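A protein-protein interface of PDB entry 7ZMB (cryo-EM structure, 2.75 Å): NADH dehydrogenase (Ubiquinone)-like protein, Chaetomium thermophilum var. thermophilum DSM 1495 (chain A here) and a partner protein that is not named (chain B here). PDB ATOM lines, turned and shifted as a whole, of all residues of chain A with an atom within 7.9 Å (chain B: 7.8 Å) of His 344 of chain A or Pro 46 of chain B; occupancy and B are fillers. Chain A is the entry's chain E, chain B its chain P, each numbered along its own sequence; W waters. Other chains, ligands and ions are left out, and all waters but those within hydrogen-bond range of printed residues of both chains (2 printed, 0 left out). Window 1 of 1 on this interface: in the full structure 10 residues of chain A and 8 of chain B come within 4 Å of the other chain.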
ATOM      1  N   GLY A 204      -6.327 -29.657  28.753  1.00  0.00           N
ATOM      2  CA  GLY A 204      -7.392 -29.643  27.774  1.00  0.00           C
ATOM      3  C   GLY A 204      -8.536 -28.798  28.287  1.00  0.00           C
ATOM      4  O   GLY A 204      -8.371 -28.011  29.215  1.00  0.00           O
ATOM      5  N   PHE A 205      -9.685 -28.957  27.649  1.00  0.00           N
ATOM      6  CA  PHE A 205     -10.911 -28.367  28.159  1.00  0.00           C
ATOM      7  C   PHE A 205     -11.238 -29.194  29.403  1.00  0.00           C
ATOM      8  O   PHE A 205     -10.932 -30.390  29.453  1.00  0.00           O
ATOM      9  CB  PHE A 205     -12.000 -28.474  27.070  1.00  0.00           C
ATOM     10  CG  PHE A 205     -13.259 -27.654  27.289  1.00  0.00           C
ATOM     11  CD1 PHE A 205     -13.258 -26.300  26.982  1.00  0.00           C
ATOM     12  CD2 PHE A 205     -14.443 -28.216  27.723  1.00  0.00           C
ATOM     13  CE1 PHE A 205     -14.406 -25.532  27.121  1.00  0.00           C
ATOM     14  CE2 PHE A 205     -15.585 -27.448  27.885  1.00  0.00           C
ATOM     15  CZ  PHE A 205     -15.562 -26.105  27.577  1.00  0.00           C
ATOM     16  N   LEU A 210      -4.775 -26.640  33.716  1.00  0.00           N
ATOM     17  CA  LEU A 210      -4.852 -25.242  33.327  1.00  0.00           C
ATOM     18  C   LEU A 210      -5.988 -24.525  34.027  1.00  0.00           C
ATOM     19  O   LEU A 210      -5.855 -23.355  34.395  1.00  0.00           O
ATOM     20  CB  LEU A 210      -5.014 -25.139  31.813  1.00  0.00           C
ATOM     21  CG  LEU A 210      -3.715 -25.032  31.027  1.00  0.00           C
ATOM     22  CD1 LEU A 210      -2.880 -26.225  31.313  1.00  0.00           C
ATOM     23  CD2 LEU A 210      -4.012 -24.959  29.546  1.00  0.00           C
ATOM     24  N   HIS A 233      -1.463 -32.932  25.793  1.00  0.00           N
ATOM     25  CA  HIS A 233      -2.841 -32.643  25.435  1.00  0.00           C
ATOM     26  C   HIS A 233      -3.703 -33.886  25.617  1.00  0.00           C
ATOM     27  O   HIS A 233      -3.334 -34.981  25.190  1.00  0.00           O
ATOM     28  CB  HIS A 233      -2.890 -32.169  23.983  1.00  0.00           C
ATOM     29  CG  HIS A 233      -4.056 -31.293  23.658  1.00  0.00           C
ATOM     30  ND1 HIS A 233      -4.400 -30.969  22.364  1.00  0.00           N
ATOM     31  CD2 HIS A 233      -4.958 -30.674  24.452  1.00  0.00           C
ATOM     32  CE1 HIS A 233      -5.461 -30.185  22.377  1.00  0.00           C
ATOM     33  NE2 HIS A 233      -5.816 -29.987  23.632  1.00  0.00           N
ATOM     34  N   ASN A 235      -6.522 -34.303  24.174  1.00  0.00           N
ATOM     35  CA  ASN A 235      -7.031 -34.628  22.848  1.00  0.00           C
ATOM     36  C   ASN A 235      -6.088 -35.571  22.118  1.00  0.00           C
ATOM     37  O   ASN A 235      -6.534 -36.487  21.420  1.00  0.00           O
ATOM     38  CB  ASN A 235      -7.250 -33.349  22.040  1.00  0.00           C
ATOM     39  CG  ASN A 235      -8.328 -32.470  22.634  1.00  0.00           C
ATOM     40  OD1 ASN A 235      -8.712 -32.644  23.782  1.00  0.00           O
ATOM     41  ND2 ASN A 235      -8.837 -31.544  21.849  1.00  0.00           N
ATOM     42  N   GLU A 275      -2.134 -15.256  29.802  1.00  0.00           N
ATOM     43  CA  GLU A 275      -3.305 -15.470  28.967  1.00  0.00           C
ATOM     44  C   GLU A 275      -4.563 -14.871  29.579  1.00  0.00           C
ATOM     45  O   GLU A 275      -5.278 -14.117  28.917  1.00  0.00           O
ATOM     46  CB  GLU A 275      -3.486 -16.966  28.717  1.00  0.00           C
ATOM     47  CG  GLU A 275      -4.279 -17.304  27.474  1.00  0.00           C
ATOM     48  CD  GLU A 275      -3.778 -16.600  26.237  1.00  0.00           C
ATOM     49  OE1 GLU A 275      -2.869 -17.138  25.575  1.00  0.00           O
ATOM     50  OE2 GLU A 275      -4.307 -15.519  25.909  1.00  0.00           O
ATOM     51  N   ILE A 338       1.861 -27.131  25.065  1.00  0.00           N
ATOM     52  CA  ILE A 338       0.776 -26.569  25.861  1.00  0.00           C
ATOM     53  C   ILE A 338       0.585 -25.083  25.578  1.00  0.00           C
ATOM     54  O   ILE A 338      -0.521 -24.555  25.732  1.00  0.00           O
ATOM     55  CB  ILE A 338       1.034 -26.841  27.357  1.00  0.00           C
ATOM     56  CG1 ILE A 338      -0.204 -26.536  28.193  1.00  0.00           C
ATOM     57  CG2 ILE A 338       2.230 -26.065  27.866  1.00  0.00           C
ATOM     58  CD1 ILE A 338      -0.124 -27.127  29.544  1.00  0.00           C
ATOM     59  N   SER A 339       1.644 -24.387  25.157  1.00  0.00           N
ATOM     60  CA  SER A 339       1.544 -22.948  24.949  1.00  0.00           C
ATOM     61  C   SER A 339       0.547 -22.612  23.847  1.00  0.00           C
ATOM     62  O   SER A 339      -0.189 -21.625  23.947  1.00  0.00           O
ATOM     63  CB  SER A 339       2.918 -22.364  24.622  1.00  0.00           C
ATOM     64  OG  SER A 339       2.857 -20.951  24.528  1.00  0.00           O
ATOM     65  N   LYS A 340       0.501 -23.425  22.793  1.00  0.00           N
ATOM     66  CA  LYS A 340      -0.407 -23.192  21.679  1.00  0.00           C
ATOM     67  C   LYS A 340      -1.868 -23.316  22.070  1.00  0.00           C
ATOM     68  O   LYS A 340      -2.735 -22.918  21.287  1.00  0.00           O
ATOM     69  CB  LYS A 340      -0.105 -24.170  20.545  1.00  0.00           C
ATOM     70  CG  LYS A 340       1.339 -24.140  20.060  1.00  0.00           C
ATOM     71  CD  LYS A 340       1.601 -22.911  19.204  1.00  0.00           C
ATOM     72  CE  LYS A 340       2.895 -23.045  18.429  1.00  0.00           C
ATOM     73  NZ  LYS A 340       4.066 -22.640  19.253  1.00  0.00           N
ATOM     74  N   TRP A 341      -2.159 -23.858  23.249  1.00  0.00           N
ATOM     75  CA  TRP A 341      -3.515 -24.170  23.664  1.00  0.00           C
ATOM     76  C   TRP A 341      -4.018 -23.287  24.789  1.00  0.00           C
ATOM     77  O   TRP A 341      -5.178 -23.416  25.183  1.00  0.00           O
ATOM     78  CB  TRP A 341      -3.591 -25.636  24.091  1.00  0.00           C
ATOM     79  CG  TRP A 341      -3.382 -26.550  22.969  1.00  0.00           C
ATOM     80  CD1 TRP A 341      -2.267 -27.277  22.700  1.00  0.00           C
ATOM     81  CD2 TRP A 341      -4.311 -26.835  21.929  1.00  0.00           C
ATOM     82  NE1 TRP A 341      -2.443 -28.003  21.551  1.00  0.00           N
ATOM     83  CE2 TRP A 341      -3.693 -27.747  21.057  1.00  0.00           C
ATOM     84  CE3 TRP A 341      -5.611 -26.409  21.652  1.00  0.00           C
ATOM     85  CZ2 TRP A 341      -4.330 -28.242  19.932  1.00  0.00           C
ATOM     86  CZ3 TRP A 341      -6.237 -26.901  20.536  1.00  0.00           C
ATOM     87  CH2 TRP A 341      -5.599 -27.810  19.690  1.00  0.00           C
ATOM     88  N   THR A 342      -3.180 -22.400  25.314  1.00  0.00           N
ATOM     89  CA  THR A 342      -3.574 -21.583  26.455  1.00  0.00           C
ATOM     90  C   THR A 342      -4.681 -20.600  26.089  1.00  0.00           C
ATOM     91  O   THR A 342      -5.589 -20.362  26.888  1.00  0.00           O
ATOM     92  CB  THR A 342      -2.356 -20.851  27.002  1.00  0.00           C
ATOM     93  OG1 THR A 342      -1.803 -20.025  25.974  1.00  0.00           O
ATOM     94  CG2 THR A 342      -1.303 -21.844  27.450  1.00  0.00           C
ATOM     95  N   TYR A 343      -4.628 -20.012  24.893  1.00  0.00           N
ATOM     96  CA  TYR A 343      -5.664 -19.056  24.521  1.00  0.00           C
ATOM     97  C   TYR A 343      -7.017 -19.734  24.383  1.00  0.00           C
ATOM     98  O   TYR A 343      -8.035 -19.207  24.843  1.00  0.00           O
ATOM     99  CB  TYR A 343      -5.312 -18.342  23.221  1.00  0.00           C
ATOM    100  CG  TYR A 343      -6.446 -17.483  22.731  1.00  0.00           C
ATOM    101  CD1 TYR A 343      -6.744 -16.283  23.354  1.00  0.00           C
ATOM    102  CD2 TYR A 343      -7.245 -17.884  21.667  1.00  0.00           C
ATOM    103  CE1 TYR A 343      -7.790 -15.495  22.919  1.00  0.00           C
ATOM    104  CE2 TYR A 343      -8.295 -17.103  21.229  1.00  0.00           C
ATOM    105  CZ  TYR A 343      -8.562 -15.913  21.860  1.00  0.00           C
ATOM    106  OH  TYR A 343      -9.601 -15.137  21.427  1.00  0.00           O
ATOM    107  N   HIS A 344      -7.048 -20.898  23.740  1.00  0.00           N
ATOM    108  CA  HIS A 344      -8.313 -21.566  23.476  1.00  0.00           C
ATOM    109  C   HIS A 344      -9.036 -21.909  24.766  1.00  0.00           C
ATOM    110  O   HIS A 344     -10.249 -21.706  24.881  1.00  0.00           O
ATOM    111  CB  HIS A 344      -8.074 -22.830  22.658  1.00  0.00           C
ATOM    112  CG  HIS A 344      -9.316 -23.378  22.036  1.00  0.00           C
ATOM    113  ND1 HIS A 344     -10.031 -24.415  22.592  1.00  0.00           N
ATOM    114  CD2 HIS A 344      -9.990 -23.011  20.922  1.00  0.00           C
ATOM    115  CE1 HIS A 344     -11.087 -24.669  21.843  1.00  0.00           C
ATOM    116  NE2 HIS A 344     -11.087 -23.830  20.824  1.00  0.00           N
ATOM    117  N   TYR A 345      -8.307 -22.434  25.750  1.00  0.00           N
ATOM    118  CA  TYR A 345      -8.918 -22.978  26.952  1.00  0.00           C
ATOM    119  C   TYR A 345      -9.006 -21.988  28.099  1.00  0.00           C
ATOM    120  O   TYR A 345      -9.790 -22.216  29.023  1.00  0.00           O
ATOM    121  CB  TYR A 345      -8.151 -24.210  27.426  1.00  0.00           C
ATOM    122  CG  TYR A 345      -8.180 -25.355  26.458  1.00  0.00           C
ATOM    123  CD1 TYR A 345      -9.346 -25.685  25.787  1.00  0.00           C
ATOM    124  CD2 TYR A 345      -7.042 -26.112  26.213  1.00  0.00           C
ATOM    125  CE1 TYR A 345      -9.378 -26.729  24.902  1.00  0.00           C
ATOM    126  CE2 TYR A 345      -7.067 -27.159  25.320  1.00  0.00           C
ATOM    127  CZ  TYR A 345      -8.238 -27.462  24.671  1.00  0.00           C
ATOM    128  OH  TYR A 345      -8.275 -28.502  23.783  1.00  0.00           O
ATOM    129  N   LEU A 346      -8.223 -20.912  28.088  1.00  0.00           N
ATOM    130  CA  LEU A 346      -8.238 -19.970  29.191  1.00  0.00           C
ATOM    131  C   LEU A 346      -9.048 -18.719  28.904  1.00  0.00           C
ATOM    132  O   LEU A 346      -9.308 -17.949  29.830  1.00  0.00           O
ATOM    133  CB  LEU A 346      -6.812 -19.566  29.579  1.00  0.00           C
ATOM    134  CG  LEU A 346      -5.911 -20.659  30.143  1.00  0.00           C
ATOM    135  CD1 LEU A 346      -4.540 -20.094  30.411  1.00  0.00           C
ATOM    136  CD2 LEU A 346      -6.504 -21.272  31.393  1.00  0.00           C
ATOM    137  N   LEU A 347      -9.466 -18.513  27.660  1.00  0.00           N
ATOM    138  CA  LEU A 347     -10.230 -17.321  27.302  1.00  0.00           C
ATOM    139  C   LEU A 347     -11.479 -17.103  28.150  1.00  0.00           C
ATOM    140  O   LEU A 347     -11.773 -15.938  28.466  1.00  0.00           O
ATOM    141  CB  LEU A 347     -10.580 -17.383  25.810  1.00  0.00           C
ATOM    142  CG  LEU A 347     -11.454 -16.262  25.255  1.00  0.00           C
ATOM    143  CD1 LEU A 347     -10.659 -14.993  25.051  1.00  0.00           C
ATOM    144  CD2 LEU A 347     -12.085 -16.717  23.966  1.00  0.00           C
ATOM    145  N   PRO A 348     -12.258 -18.128  28.534  1.00  0.00           N
ATOM    146  CA  PRO A 348     -13.373 -17.895  29.465  1.00  0.00           C
ATOM    147  C   PRO A 348     -12.981 -17.212  30.764  1.00  0.00           C
ATOM    148  O   PRO A 348     -13.846 -16.734  31.495  1.00  0.00           O
ATOM    149  CB  PRO A 348     -13.886 -19.310  29.745  1.00  0.00           C
ATOM    150  CG  PRO A 348     -13.547 -20.065  28.564  1.00  0.00           C
ATOM    151  CD  PRO A 348     -12.327 -19.477  27.949  1.00  0.00           C
ATOM    152  N   TYR A 349     -11.695 -17.172  31.086  1.00  0.00           N
ATOM    153  CA  TYR A 349     -11.244 -16.627  32.356  1.00  0.00           C
ATOM    154  C   TYR A 349     -10.558 -15.281  32.204  1.00  0.00           C
ATOM    155  O   TYR A 349      -9.990 -14.774  33.172  1.00  0.00           O
ATOM    156  CB  TYR A 349     -10.334 -17.633  33.070  1.00  0.00           C
ATOM    157  CG  TYR A 349     -10.981 -18.987  33.274  1.00  0.00           C
ATOM    158  CD1 TYR A 349     -11.257 -19.821  32.201  1.00  0.00           C
ATOM    159  CD2 TYR A 349     -11.334 -19.421  34.540  1.00  0.00           C
ATOM    160  CE1 TYR A 349     -11.858 -21.043  32.378  1.00  0.00           C
ATOM    161  CE2 TYR A 349     -11.935 -20.653  34.731  1.00  0.00           C
ATOM    162  CZ  TYR A 349     -12.195 -21.456  33.642  1.00  0.00           C
ATOM    163  OH  TYR A 349     -12.793 -22.680  33.816  1.00  0.00           O
ATOM    164  N   PRO A 358      -6.287 -10.403  21.162  1.00  0.00           N
ATOM    165  CA  PRO A 358      -5.883 -11.605  20.431  1.00  0.00           C
ATOM    166  C   PRO A 358      -5.097 -12.543  21.327  1.00  0.00           C
ATOM    167  O   PRO A 358      -4.733 -12.175  22.452  1.00  0.00           O
ATOM    168  CB  PRO A 358      -5.007 -11.050  19.291  1.00  0.00           C
ATOM    169  CG  PRO A 358      -5.216  -9.586  19.297  1.00  0.00           C
ATOM    170  CD  PRO A 358      -5.557  -9.218  20.689  1.00  0.00           C
ATOM    171  N   PRO A 359      -4.833 -13.769  20.875  1.00  0.00           N
ATOM    172  CA  PRO A 359      -4.032 -14.689  21.684  1.00  0.00           C
ATOM    173  C   PRO A 359      -2.647 -14.123  21.953  1.00  0.00           C
ATOM    174  O   PRO A 359      -2.076 -13.401  21.132  1.00  0.00           O
ATOM    175  CB  PRO A 359      -3.964 -15.950  20.821  1.00  0.00           C
ATOM    176  CG  PRO A 359      -5.127 -15.847  19.920  1.00  0.00           C
ATOM    177  CD  PRO A 359      -5.295 -14.409  19.633  1.00  0.00           C
ATOM    178  N   SER A 360      -2.116 -14.465  23.127  1.00  0.00           N
ATOM    179  CA  SER A 360      -0.889 -13.841  23.608  1.00  0.00           C
ATOM    180  C   SER A 360       0.265 -14.043  22.634  1.00  0.00           C
ATOM    181  O   SER A 360       0.990 -13.093  22.314  1.00  0.00           O
ATOM    182  CB  SER A 360      -0.528 -14.403  24.979  1.00  0.00           C
ATOM    183  OG  SER A 360      -0.135 -15.756  24.872  1.00  0.00           O
ATOM    184  N   THR A 361       0.460 -15.282  22.169  1.00  0.00           N
ATOM    185  CA  THR A 361       1.529 -15.696  21.258  1.00  0.00           C
ATOM    186  C   THR A 361       2.865 -15.022  21.570  1.00  0.00           C
ATOM    187  O   THR A 361       3.642 -14.709  20.660  1.00  0.00           O
ATOM    188  CB  THR A 361       1.128 -15.468  19.787  1.00  0.00           C
ATOM    189  OG1 THR A 361       2.115 -16.053  18.928  1.00  0.00           O
ATOM    190  CG2 THR A 361       0.969 -13.985  19.431  1.00  0.00           C
ATOM    191  N   GLN B  40     -10.417 -12.348  13.536  1.00  0.00           N
ATOM    192  CA  GLN B  40      -9.826 -13.229  14.536  1.00  0.00           C
ATOM    193  C   GLN B  40     -10.393 -12.959  15.921  1.00  0.00           C
ATOM    194  O   GLN B  40     -10.674 -13.895  16.678  1.00  0.00           O
ATOM    195  CB  GLN B  40      -8.308 -13.073  14.526  1.00  0.00           C
ATOM    196  CG  GLN B  40      -7.594 -13.994  15.477  1.00  0.00           C
ATOM    197  CD  GLN B  40      -6.182 -13.562  15.771  1.00  0.00           C
ATOM    198  OE1 GLN B  40      -5.941 -12.470  16.271  1.00  0.00           O
ATOM    199  NE2 GLN B  40      -5.235 -14.424  15.462  1.00  0.00           N
ATOM    200  N   TYR B  43     -14.366 -13.756  16.145  1.00  0.00           N
ATOM    201  CA  TYR B  43     -14.695 -15.168  16.190  1.00  0.00           C
ATOM    202  C   TYR B  43     -13.767 -15.953  17.100  1.00  0.00           C
ATOM    203  O   TYR B  43     -13.841 -17.183  17.125  1.00  0.00           O
ATOM    204  CB  TYR B  43     -14.683 -15.732  14.774  1.00  0.00           C
ATOM    205  CG  TYR B  43     -15.822 -15.183  13.958  1.00  0.00           C
ATOM    206  CD1 TYR B  43     -17.133 -15.509  14.261  1.00  0.00           C
ATOM    207  CD2 TYR B  43     -15.593 -14.290  12.928  1.00  0.00           C
ATOM    208  CE1 TYR B  43     -18.173 -14.993  13.541  1.00  0.00           C
ATOM    209  CE2 TYR B  43     -16.631 -13.764  12.207  1.00  0.00           C
ATOM    210  CZ  TYR B  43     -17.919 -14.120  12.518  1.00  0.00           C
ATOM    211  OH  TYR B  43     -18.956 -13.605  11.793  1.00  0.00           O
ATOM    212  N   SER B  44     -12.905 -15.264  17.852  1.00  0.00           N
ATOM    213  CA  SER B  44     -11.997 -15.895  18.808  1.00  0.00           C
ATOM    214  C   SER B  44     -11.183 -17.001  18.149  1.00  0.00           C
ATOM    215  O   SER B  44     -11.013 -18.092  18.694  1.00  0.00           O
ATOM    216  CB  SER B  44     -12.758 -16.420  20.025  1.00  0.00           C
ATOM    217  OG  SER B  44     -13.117 -15.357  20.888  1.00  0.00           O
ATOM    218  N   ILE B  45     -10.673 -16.714  16.964  1.00  0.00           N
ATOM    219  CA  ILE B  45      -9.852 -17.693  16.249  1.00  0.00           C
ATOM    220  C   ILE B  45      -8.559 -17.914  17.021  1.00  0.00           C
ATOM    221  O   ILE B  45      -7.859 -16.940  17.339  1.00  0.00           O
ATOM    222  CB  ILE B  45      -9.572 -17.214  14.828  1.00  0.00           C
ATOM    223  CG1 ILE B  45     -10.879 -16.833  14.146  1.00  0.00           C
ATOM    224  CG2 ILE B  45      -8.869 -18.301  14.032  1.00  0.00           C
ATOM    225  CD1 ILE B  45     -11.836 -17.977  14.025  1.00  0.00           C
ATOM    226  N   PRO B  46      -8.207 -19.157  17.356  1.00  0.00           N
ATOM    227  CA  PRO B  46      -6.962 -19.410  18.086  1.00  0.00           C
ATOM    228  C   PRO B  46      -5.743 -19.533  17.192  1.00  0.00           C
ATOM    229  O   PRO B  46      -4.617 -19.436  17.694  1.00  0.00           O
ATOM    230  CB  PRO B  46      -7.260 -20.728  18.818  1.00  0.00           C
ATOM    231  CG  PRO B  46      -8.371 -21.366  18.064  1.00  0.00           C
ATOM    232  CD  PRO B  46      -8.970 -20.388  17.110  1.00  0.00           C
ATOM    233  N   PHE B  47      -5.944 -19.741  15.894  1.00  0.00           N
ATOM    234  CA  PHE B  47      -4.878 -19.635  14.922  1.00  0.00           C
ATOM    235  C   PHE B  47      -4.459 -18.179  14.751  1.00  0.00           C
ATOM    236  O   PHE B  47      -5.215 -17.263  15.078  1.00  0.00           O
ATOM    237  CB  PHE B  47      -5.328 -20.198  13.578  1.00  0.00           C
ATOM    238  CG  PHE B  47      -5.297 -21.692  13.499  1.00  0.00           C
ATOM    239  CD1 PHE B  47      -4.555 -22.437  14.404  1.00  0.00           C
ATOM    240  CD2 PHE B  47      -5.990 -22.358  12.490  1.00  0.00           C
ATOM    241  CE1 PHE B  47      -4.521 -23.823  14.311  1.00  0.00           C
ATOM    242  CE2 PHE B  47      -5.960 -23.730  12.391  1.00  0.00           C
ATOM    243  CZ  PHE B  47      -5.226 -24.468  13.305  1.00  0.00           C
ATOM    244  N   PRO B  48      -3.250 -17.943  14.254  1.00  0.00           N
ATOM    245  CA  PRO B  48      -2.845 -16.578  13.915  1.00  0.00           C
ATOM    246  C   PRO B  48      -3.411 -16.129  12.578  1.00  0.00           C
ATOM    247  O   PRO B  48      -3.774 -16.929  11.716  1.00  0.00           O
ATOM    248  CB  PRO B  48      -1.316 -16.660  13.868  1.00  0.00           C
ATOM    249  CG  PRO B  48      -1.033 -18.057  13.561  1.00  0.00           C
ATOM    250  CD  PRO B  48      -2.111 -18.871  14.217  1.00  0.00           C
ATOM    251  N   VAL B  49      -3.443 -14.806  12.413  1.00  0.00           N
ATOM    252  CA  VAL B  49      -4.053 -14.174  11.250  1.00  0.00           C
ATOM    253  C   VAL B  49      -3.377 -14.589   9.945  1.00  0.00           C
ATOM    254  O   VAL B  49      -4.000 -14.533   8.878  1.00  0.00           O
ATOM    255  CB  VAL B  49      -4.041 -12.645  11.466  1.00  0.00           C
ATOM    256  CG1 VAL B  49      -4.297 -11.888  10.179  1.00  0.00           C
ATOM    257  CG2 VAL B  49      -5.063 -12.271  12.513  1.00  0.00           C
ATOM    258  N   HIS B  51      -2.665 -17.601   8.950  1.00  0.00           N
ATOM    259  CA  HIS B  51      -3.440 -18.715   8.419  1.00  0.00           C
ATOM    260  C   HIS B  51      -4.746 -18.250   7.794  1.00  0.00           C
ATOM    261  O   HIS B  51      -5.171 -18.788   6.767  1.00  0.00           O
ATOM    262  CB  HIS B  51      -3.722 -19.740   9.513  1.00  0.00           C
ATOM    263  CG  HIS B  51      -2.497 -20.410  10.047  1.00  0.00           C
ATOM    264  ND1 HIS B  51      -1.958 -20.098  11.276  1.00  0.00           N
ATOM    265  CD2 HIS B  51      -1.703 -21.368   9.518  1.00  0.00           C
ATOM    266  CE1 HIS B  51      -0.885 -20.841  11.483  1.00  0.00           C
ATOM    267  NE2 HIS B  51      -0.709 -21.620  10.432  1.00  0.00           N
ATOM    268  N   ILE B  52      -5.414 -17.276   8.415  1.00  0.00           N
ATOM    269  CA  ILE B  52      -6.687 -16.794   7.893  1.00  0.00           C
ATOM    270  C   ILE B  52      -6.491 -16.158   6.526  1.00  0.00           C
ATOM    271  O   ILE B  52      -7.271 -16.391   5.597  1.00  0.00           O
ATOM    272  CB  ILE B  52      -7.336 -15.810   8.889  1.00  0.00           C
ATOM    273  CG1 ILE B  52      -7.626 -16.496  10.219  1.00  0.00           C
ATOM    274  CG2 ILE B  52      -8.608 -15.212   8.314  1.00  0.00           C
ATOM    275  CD1 ILE B  52      -7.714 -15.545  11.388  1.00  0.00           C
ATOM    276  N   GLN B  93     -19.117 -18.742  15.305  1.00  0.00           N
ATOM    277  CA  GLN B  93     -17.798 -19.363  15.307  1.00  0.00           C
ATOM    278  C   GLN B  93     -17.806 -20.700  14.581  1.00  0.00           C
ATOM    279  O   GLN B  93     -16.870 -21.014  13.842  1.00  0.00           O
ATOM    280  CB  GLN B  93     -17.290 -19.531  16.734  1.00  0.00           C
ATOM    281  CG  GLN B  93     -15.846 -19.967  16.799  1.00  0.00           C
ATOM    282  CD  GLN B  93     -15.487 -20.589  18.111  1.00  0.00           C
ATOM    283  OE1 GLN B  93     -16.102 -21.558  18.541  1.00  0.00           O
ATOM    284  NE2 GLN B  93     -14.475 -20.037  18.765  1.00  0.00           N
ATOM    285  N   MET B  97     -15.329 -21.597  11.705  1.00  0.00           N
ATOM    286  CA  MET B  97     -14.460 -22.760  11.841  1.00  0.00           C
ATOM    287  C   MET B  97     -14.820 -23.883  10.879  1.00  0.00           C
ATOM    288  O   MET B  97     -13.957 -24.707  10.564  1.00  0.00           O
ATOM    289  CB  MET B  97     -14.466 -23.295  13.275  1.00  0.00           C
ATOM    290  CG  MET B  97     -14.119 -22.281  14.340  1.00  0.00           C
ATOM    291  SD  MET B  97     -12.428 -21.687  14.234  1.00  0.00           S
ATOM    292  CE  MET B  97     -11.523 -23.214  14.448  1.00  0.00           C
HETATM  293  O   HOH W   1     -11.821 -22.753  17.746  1.00  0.00           O
HETATM  294  O   HOH W   2      -8.526 -14.426  18.646  1.00  0.00           O
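Of the 22 printed residues of chain A, 5 touch a printed residue of chain B. Among the printed residues, 8 pairs touch across the chains.
Ser 44 of chain B touches Tyr 343 of chain A (OG to OH, 3.6 Å). CE2 of Tyr 343 of chain A touches O of Ile 45 of chain B, at 3.9 Å. CD2 of Tyr 343 of chain A touches CA of Pro 46 of chain B, at 3.9 Å. CD2 of His 344 of chain A touches CG of Pro 46 of chain B, at 3.7 Å. Leu 347 of chain A touches Ser 44 of chain B. Gln 40 of chain B touches Pro 358 of chain A (OE1 to CB, 3.5 Å). OE1 of Gln 40 of chain B touches CD of Pro 359 of chain A (3.9 Å). CG of Pro 359 of chain A touches O of Ile 45 of chain B, at 3.9 Å.
His 344 of chain A touches just one residue of chain B: Pro 46. Pro 46 of chain B touches two residues of chain A. Printed residues of chain B within 4 Å of Leu 347 of chain A: Ser 44. Of the printed residues of chain B, Pro 359 of chain A touches Gln 40 (3.9 Å) and Ile 45 (3.9 Å). Of the printed residues of chain B, Tyr 343 of chain A touches Ser 44 (3.6 Å), Ile 45 (3.9 Å) and Pro 46 (3.9 Å). Of the printed residues of chain B, Pro 358 of chain A touches Gln 40. Printed residues of chain A within 4 Å of Gln 40 of chain B: Pro 358 and Pro 359. Ser 360 of chain A touches none of the printed residues of chain B. Val 49 of chain B touches none of the printed residues of chain A. The nearest printed residue of chain B that does not touch His 344 of chain A is Gln 93 of chain B (5.5 Å). The nearest printed residue of chain A that does not touch Gln 40 of chain B is Tyr 343 of chain A (5.0 Å).
The backbone NH of Tyr 343 of chain A lies within hydrogen-bond range of the side-chain carboxylate of Glu 275 of chain A (3.4 Å). N of Ile 45 of chain B is in hydrogen-bond range of O of Gln 40 of chain B. O of Phe 47 of chain B lies within hydrogen-bond range of NE2 of Gln 40 of chain B, 2.9 Å away.
Water W2 lies within hydrogen-bond range of O of Ile 45 of chain B, O of Gln 40 of chain B and OH of Tyr 343 of chain A. Water W1 lies within hydrogen-bond range of a ring nitrogen (NE2) of His 344 of chain A (3.3 Å) and the side-chain sulfur of Met 97 of chain B (3.7 Å).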
